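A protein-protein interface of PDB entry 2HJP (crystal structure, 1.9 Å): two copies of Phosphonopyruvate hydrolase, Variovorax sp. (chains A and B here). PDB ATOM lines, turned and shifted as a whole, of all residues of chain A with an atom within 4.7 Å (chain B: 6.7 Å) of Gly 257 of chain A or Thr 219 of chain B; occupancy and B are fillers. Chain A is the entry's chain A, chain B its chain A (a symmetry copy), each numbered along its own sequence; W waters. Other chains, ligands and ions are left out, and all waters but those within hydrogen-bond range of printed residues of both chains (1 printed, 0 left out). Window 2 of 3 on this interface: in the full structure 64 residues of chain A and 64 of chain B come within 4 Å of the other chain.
The backbone carbonyl oxygen (O) of Gly 257 of chain A lies within hydrogen-bond range of the backbone NH (N) of Glu 220 of chain B, 3.0 Å away.
Water W1 lies within hydrogen-bond range of O of Gly 257 of chain A (2.7 Å), N of Ala 221 of chain B (3.1 Å) and N of Glu 220 of chain B (3.5 Å).
Gly 257 of chain A touches two residues of chain B.
Of the printed residues of chain B, Arg 260 of chain A touches Pro 216 (3.4 Å).
Printed residues of chain A within 4 Å of Pro 216 of chain B: Arg 260.
Thr 219 of chain B touches just one residue of chain A: Gly 257.
Of the printed residues of chain A, Glu 220 of chain B touches Gly 257.
Ala 221 of chain B touches none of the printed residues of chain A.
Of the printed residues of chain A, Tyr 234 of chain B touches Gly 258 (3.6 Å).
The nearest residue of chain A that does not touch Thr 219 of chain B is Arg 260 of chain A (4.2 Å).
The nearest printed residue of chain A that does not touch Pro 216 of chain B is Gly 258 of chain A (5.9 Å).
No position is printed for both chains.
Of the 4 pairs that touch across the chains among the printed residues, none has its exchanged pair printed and touching as well.
Hydrophobic or aromatic side chains of chain B within 4 Å of the printed part of chain A: Tyr 234.
Of the 8 printed residues of chain A, 3 touch a printed residue of chain B.
Among the printed residues, no Asp or Glu carboxylate lies within 4 Å of a Lys or Arg side-chain nitrogen of the other chain.
Among the printed residues, pairs that only touch across the chains: Gly 257 of chain A with Thr 219 of chain B (3.95 Å), Gly 258 of chain A with Tyr 234 of chain B (3.6 Å) and Arg 260 of chain A with Pro 216 of chain B (3.4 Å).
N of Asp 222 of chain B sits at hydrogen-bond distance from OG1 of Thr 219 of chain B, 3.1 Å away.
The side-chain hydroxyl of Thr 219 of chain B lies close to the backbone NH of Ala 221 of chain B, 3.2 Å away.
OE1 of Glu 220 of chain B is in hydrogen-bond range of OH of Tyr 234 of chain B, at 2.5 Å.
O of Ile 253 of chain A sits at hydrogen-bond distance from N of Gly 258 of chain A.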
ATOM      1  N   ARG A 252       8.143  24.080   6.803  1.00  0.00           N
ATOM      2  CA  ARG A 252       6.972  23.227   6.913  1.00  0.00           C
ATOM      3  C   ARG A 252       5.681  24.025   7.081  1.00  0.00           C
ATOM      4  O   ARG A 252       4.650  23.700   6.443  1.00  0.00           O
ATOM      5  CB  ARG A 252       7.075  22.244   8.088  1.00  0.00           C
ATOM      6  CG  ARG A 252       8.150  21.181   7.865  1.00  0.00           C
ATOM      7  CD  ARG A 252       8.390  20.219   9.041  1.00  0.00           C
ATOM      8  NE  ARG A 252       7.195  19.419   9.373  1.00  0.00           N
ATOM      9  CZ  ARG A 252       6.984  18.807  10.554  1.00  0.00           C
ATOM     10  NH1 ARG A 252       7.884  18.907  11.564  1.00  0.00           N
ATOM     11  NH2 ARG A 252       5.887  18.065  10.714  1.00  0.00           N
ATOM     12  N   ILE A 253       5.708  25.061   7.931  1.00  0.00           N
ATOM     13  CA  ILE A 253       4.507  25.859   8.177  1.00  0.00           C
ATOM     14  C   ILE A 253       4.047  26.505   6.873  1.00  0.00           C
ATOM     15  O   ILE A 253       2.874  26.544   6.583  1.00  0.00           O
ATOM     16  CB  ILE A 253       4.776  26.937   9.304  1.00  0.00           C
ATOM     17  CG1 ILE A 253       4.846  26.251  10.690  1.00  0.00           C
ATOM     18  CG2 ILE A 253       3.641  27.982   9.371  1.00  0.00           C
ATOM     19  CD1 ILE A 253       5.692  25.003  10.849  1.00  0.00           C
ATOM     20  N   ARG A 254       4.993  26.965   6.066  1.00  0.00           N
ATOM     21  CA  ARG A 254       4.641  27.614   4.805  1.00  0.00           C
ATOM     22  C   ARG A 254       4.132  26.608   3.740  1.00  0.00           C
ATOM     23  O   ARG A 254       3.227  26.933   2.969  1.00  0.00           O
ATOM     24  CB  ARG A 254       5.829  28.479   4.340  1.00  0.00           C
ATOM     25  CG  ARG A 254       5.520  29.982   4.811  1.00  0.00           C
ATOM     26  CD  ARG A 254       4.363  30.556   4.032  1.00  0.00           C
ATOM     27  NE  ARG A 254       4.849  31.685   3.218  1.00  0.00           N
ATOM     28  CZ  ARG A 254       4.683  31.847   1.898  1.00  0.00           C
ATOM     29  NH1 ARG A 254       5.676  31.647   1.027  1.00  0.00           N
ATOM     30  NH2 ARG A 254       3.492  32.231   1.445  1.00  0.00           N
ATOM     31  N   ARG A 255       4.681  25.400   3.746  1.00  0.00           N
ATOM     32  CA  ARG A 255       4.291  24.328   2.834  1.00  0.00           C
ATOM     33  C   ARG A 255       2.906  23.800   3.275  1.00  0.00           C
ATOM     34  O   ARG A 255       2.010  23.588   2.446  1.00  0.00           O
ATOM     35  CB  ARG A 255       5.369  23.232   2.951  1.00  0.00           C
ATOM     36  CG  ARG A 255       5.559  22.285   1.828  1.00  0.00           C
ATOM     37  CD  ARG A 255       7.031  21.760   1.850  1.00  0.00           C
ATOM     38  NE  ARG A 255       7.376  21.182   3.147  1.00  0.00           N
ATOM     39  CZ  ARG A 255       8.571  21.295   3.727  1.00  0.00           C
ATOM     40  NH1 ARG A 255       9.548  21.984   3.140  1.00  0.00           N
ATOM     41  NH2 ARG A 255       8.819  20.655   4.874  1.00  0.00           N
ATOM     42  N   ASP A 256       2.709  23.596   4.577  1.00  0.00           N
ATOM     43  CA  ASP A 256       1.425  23.097   5.096  1.00  0.00           C
ATOM     44  C   ASP A 256       0.310  24.174   5.200  1.00  0.00           C
ATOM     45  O   ASP A 256      -0.869  23.857   5.413  1.00  0.00           O
ATOM     46  CB  ASP A 256       1.590  22.535   6.494  1.00  0.00           C
ATOM     47  CG  ASP A 256       2.518  21.359   6.560  1.00  0.00           C
ATOM     48  OD1 ASP A 256       2.924  20.810   5.521  1.00  0.00           O
ATOM     49  OD2 ASP A 256       2.830  21.008   7.688  1.00  0.00           O
ATOM     50  N   GLY A 257       0.679  25.440   5.076  1.00  0.00           N
ATOM     51  CA  GLY A 257      -0.317  26.480   5.199  1.00  0.00           C
ATOM     52  C   GLY A 257      -0.830  26.484   6.617  1.00  0.00           C
ATOM     53  O   GLY A 257      -2.017  26.543   6.839  1.00  0.00           O
ATOM     54  N   GLY A 258       0.057  26.401   7.591  1.00  0.00           N
ATOM     55  CA  GLY A 258      -0.425  26.403   8.968  1.00  0.00           C
ATOM     56  C   GLY A 258       0.434  25.574   9.910  1.00  0.00           C
ATOM     57  O   GLY A 258       1.437  25.046   9.475  1.00  0.00           O
ATOM     58  N   ARG A 260      -1.014  23.045  11.935  1.00  0.00           N
ATOM     59  CA  ARG A 260      -1.770  21.838  12.327  1.00  0.00           C
ATOM     60  C   ARG A 260      -0.928  20.566  12.436  1.00  0.00           C
ATOM     61  O   ARG A 260      -1.217  19.753  13.297  1.00  0.00           O
ATOM     62  CB  ARG A 260      -2.964  21.588  11.365  1.00  0.00           C
ATOM     63  CG  ARG A 260      -3.752  20.276  11.598  1.00  0.00           C
ATOM     64  CD  ARG A 260      -4.879  20.078  10.519  1.00  0.00           C
ATOM     65  N   LEU B  16      -4.899  37.664   3.164  1.00  0.00           N
ATOM     66  CA  LEU B  16      -4.613  37.271   4.549  1.00  0.00           C
ATOM     67  C   LEU B  16      -3.092  37.427   4.739  1.00  0.00           C
ATOM     68  O   LEU B  16      -2.293  36.797   4.000  1.00  0.00           O
ATOM     69  CB  LEU B  16      -4.985  35.809   4.762  1.00  0.00           C
ATOM     70  CG  LEU B  16      -4.663  35.147   6.092  1.00  0.00           C
ATOM     71  CD1 LEU B  16      -5.178  36.008   7.235  1.00  0.00           C
ATOM     72  CD2 LEU B  16      -5.339  33.725   6.085  1.00  0.00           C
ATOM     73  N   PRO B 212      -3.713  31.683  16.579  1.00  0.00           N
ATOM     74  CA  PRO B 212      -4.206  30.305  16.739  1.00  0.00           C
ATOM     75  C   PRO B 212      -3.339  29.284  17.438  1.00  0.00           C
ATOM     76  O   PRO B 212      -3.557  28.107  17.261  1.00  0.00           O
ATOM     77  CB  PRO B 212      -4.494  29.881  15.306  1.00  0.00           C
ATOM     78  CG  PRO B 212      -3.348  30.534  14.537  1.00  0.00           C
ATOM     79  CD  PRO B 212      -3.215  31.910  15.194  1.00  0.00           C
ATOM     80  N   TYR B 215      -5.179  26.620  19.316  1.00  0.00           N
ATOM     81  CA  TYR B 215      -6.121  25.849  18.502  1.00  0.00           C
ATOM     82  C   TYR B 215      -5.492  25.713  17.113  1.00  0.00           C
ATOM     83  O   TYR B 215      -6.014  26.254  16.117  1.00  0.00           O
ATOM     84  CB  TYR B 215      -7.518  26.589  18.513  1.00  0.00           C
ATOM     85  CG  TYR B 215      -7.539  28.140  18.343  1.00  0.00           C
ATOM     86  CD1 TYR B 215      -7.116  29.013  19.355  1.00  0.00           C
ATOM     87  CD2 TYR B 215      -7.930  28.705  17.117  1.00  0.00           C
ATOM     88  CE1 TYR B 215      -7.057  30.435  19.127  1.00  0.00           C
ATOM     89  CE2 TYR B 215      -7.887  30.049  16.878  1.00  0.00           C
ATOM     90  CZ  TYR B 215      -7.435  30.931  17.873  1.00  0.00           C
ATOM     91  OH  TYR B 215      -7.311  32.273  17.488  1.00  0.00           O
ATOM     92  N   PRO B 216      -4.379  24.935  17.015  1.00  0.00           N
ATOM     93  CA  PRO B 216      -3.680  24.757  15.749  1.00  0.00           C
ATOM     94  C   PRO B 216      -4.433  24.111  14.644  1.00  0.00           C
ATOM     95  O   PRO B 216      -3.959  24.088  13.566  1.00  0.00           O
ATOM     96  CB  PRO B 216      -2.450  23.938  16.126  1.00  0.00           C
ATOM     97  CG  PRO B 216      -2.960  23.049  17.176  1.00  0.00           C
ATOM     98  CD  PRO B 216      -3.841  23.994  18.021  1.00  0.00           C
ATOM     99  N   GLN B 217      -5.596  23.573  14.916  1.00  0.00           N
ATOM    100  CA  GLN B 217      -6.333  22.924  13.855  1.00  0.00           C
ATOM    101  C   GLN B 217      -7.039  23.926  12.923  1.00  0.00           C
ATOM    102  O   GLN B 217      -7.530  23.551  11.852  1.00  0.00           O
ATOM    103  CB  GLN B 217      -7.305  21.893  14.448  1.00  0.00           C
ATOM    104  CG  GLN B 217      -8.326  22.387  15.436  1.00  0.00           C
ATOM    105  CD  GLN B 217      -7.880  22.458  16.899  1.00  0.00           C
ATOM    106  OE1 GLN B 217      -8.363  21.698  17.751  1.00  0.00           O
ATOM    107  NE2 GLN B 217      -7.008  23.380  17.205  1.00  0.00           N
ATOM    108  N   LEU B 218      -7.032  25.203  13.302  1.00  0.00           N
ATOM    109  CA  LEU B 218      -7.636  26.228  12.448  1.00  0.00           C
ATOM    110  C   LEU B 218      -6.522  26.595  11.491  1.00  0.00           C
ATOM    111  O   LEU B 218      -5.622  27.373  11.837  1.00  0.00           O
ATOM    112  CB  LEU B 218      -8.046  27.432  13.284  1.00  0.00           C
ATOM    113  CG  LEU B 218      -8.862  28.447  12.477  1.00  0.00           C
ATOM    114  CD1 LEU B 218     -10.290  27.845  12.199  1.00  0.00           C
ATOM    115  CD2 LEU B 218      -8.956  29.773  13.273  1.00  0.00           C
ATOM    116  N   THR B 219      -6.572  26.064  10.278  1.00  0.00           N
ATOM    117  CA  THR B 219      -5.504  26.295   9.319  1.00  0.00           C
ATOM    118  C   THR B 219      -5.584  27.631   8.563  1.00  0.00           C
ATOM    119  O   THR B 219      -6.577  28.386   8.693  1.00  0.00           O
ATOM    120  CB  THR B 219      -5.474  25.235   8.242  1.00  0.00           C
ATOM    121  OG1 THR B 219      -6.579  25.434   7.369  1.00  0.00           O
ATOM    122  CG2 THR B 219      -5.501  23.844   8.831  1.00  0.00           C
ATOM    123  N   GLU B 220      -4.573  27.933   7.734  1.00  0.00           N
ATOM    124  CA  GLU B 220      -4.718  29.201   7.007  1.00  0.00           C
ATOM    125  C   GLU B 220      -5.888  29.160   6.015  1.00  0.00           C
ATOM    126  O   GLU B 220      -6.552  30.189   5.759  1.00  0.00           O
ATOM    127  CB  GLU B 220      -3.440  29.586   6.247  1.00  0.00           C
ATOM    128  CG  GLU B 220      -2.319  29.966   7.248  1.00  0.00           C
ATOM    129  CD  GLU B 220      -0.961  30.295   6.608  1.00  0.00           C
ATOM    130  OE1 GLU B 220       0.013  30.477   7.386  1.00  0.00           O
ATOM    131  OE2 GLU B 220      -0.869  30.376   5.376  1.00  0.00           O
ATOM    132  N   ALA B 221      -6.168  27.971   5.474  1.00  0.00           N
ATOM    133  CA  ALA B 221      -7.282  27.863   4.521  1.00  0.00           C
ATOM    134  C   ALA B 221      -8.566  28.085   5.334  1.00  0.00           C
ATOM    135  O   ALA B 221      -9.509  28.728   4.854  1.00  0.00           O
ATOM    136  CB  ALA B 221      -7.264  26.480   3.837  1.00  0.00           C
ATOM    137  N   ASP B 222      -8.608  27.584   6.567  1.00  0.00           N
ATOM    138  CA  ASP B 222      -9.797  27.820   7.349  1.00  0.00           C
ATOM    139  C   ASP B 222      -9.913  29.345   7.655  1.00  0.00           C
ATOM    140  O   ASP B 222     -11.004  29.907   7.665  1.00  0.00           O
ATOM    141  CB  ASP B 222      -9.766  27.066   8.683  1.00  0.00           C
ATOM    142  CG  ASP B 222      -9.837  25.569   8.507  1.00  0.00           C
ATOM    143  OD1 ASP B 222     -10.375  25.135   7.471  1.00  0.00           O
ATOM    144  OD2 ASP B 222      -9.348  24.861   9.404  1.00  0.00           O
ATOM    145  N   ILE B 223      -8.778  29.993   7.938  1.00  0.00           N
ATOM    146  CA  ILE B 223      -8.816  31.413   8.286  1.00  0.00           C
ATOM    147  C   ILE B 223      -9.122  32.251   7.055  1.00  0.00           C
ATOM    148  O   ILE B 223      -9.811  33.214   7.163  1.00  0.00           O
ATOM    149  CB  ILE B 223      -7.489  31.854   8.944  1.00  0.00           C
ATOM    150  CG1 ILE B 223      -7.449  31.225  10.367  1.00  0.00           C
ATOM    151  CG2 ILE B 223      -7.428  33.400   9.157  1.00  0.00           C
ATOM    152  CD1 ILE B 223      -6.069  31.207  11.023  1.00  0.00           C
ATOM    153  N   ALA B 224      -8.591  31.893   5.903  1.00  0.00           N
ATOM    154  CA  ALA B 224      -8.869  32.645   4.660  1.00  0.00           C
ATOM    155  C   ALA B 224     -10.388  32.721   4.424  1.00  0.00           C
ATOM    156  O   ALA B 224     -10.863  33.709   3.891  1.00  0.00           O
ATOM    157  CB  ALA B 224      -8.212  31.972   3.433  1.00  0.00           C
ATOM    158  N   TYR B 234       1.692  33.578  14.145  1.00  0.00           N
ATOM    159  CA  TYR B 234       2.236  32.331  14.734  1.00  0.00           C
ATOM    160  C   TYR B 234       2.994  32.843  15.937  1.00  0.00           C
ATOM    161  O   TYR B 234       4.101  33.407  15.853  1.00  0.00           O
ATOM    162  CB  TYR B 234       3.036  31.628  13.676  1.00  0.00           C
ATOM    163  CG  TYR B 234       2.065  31.149  12.596  1.00  0.00           C
ATOM    164  CD1 TYR B 234       1.085  30.219  12.896  1.00  0.00           C
ATOM    165  CD2 TYR B 234       2.120  31.665  11.299  1.00  0.00           C
ATOM    166  CE1 TYR B 234       0.158  29.795  11.913  1.00  0.00           C
ATOM    167  CE2 TYR B 234       1.205  31.258  10.288  1.00  0.00           C
ATOM    168  CZ  TYR B 234       0.227  30.317  10.630  1.00  0.00           C
ATOM    169  OH  TYR B 234      -0.677  29.930   9.684  1.00  0.00           O
HETATM  170  O   HOH W   1      -3.910  25.944   4.951  1.00  0.00           O
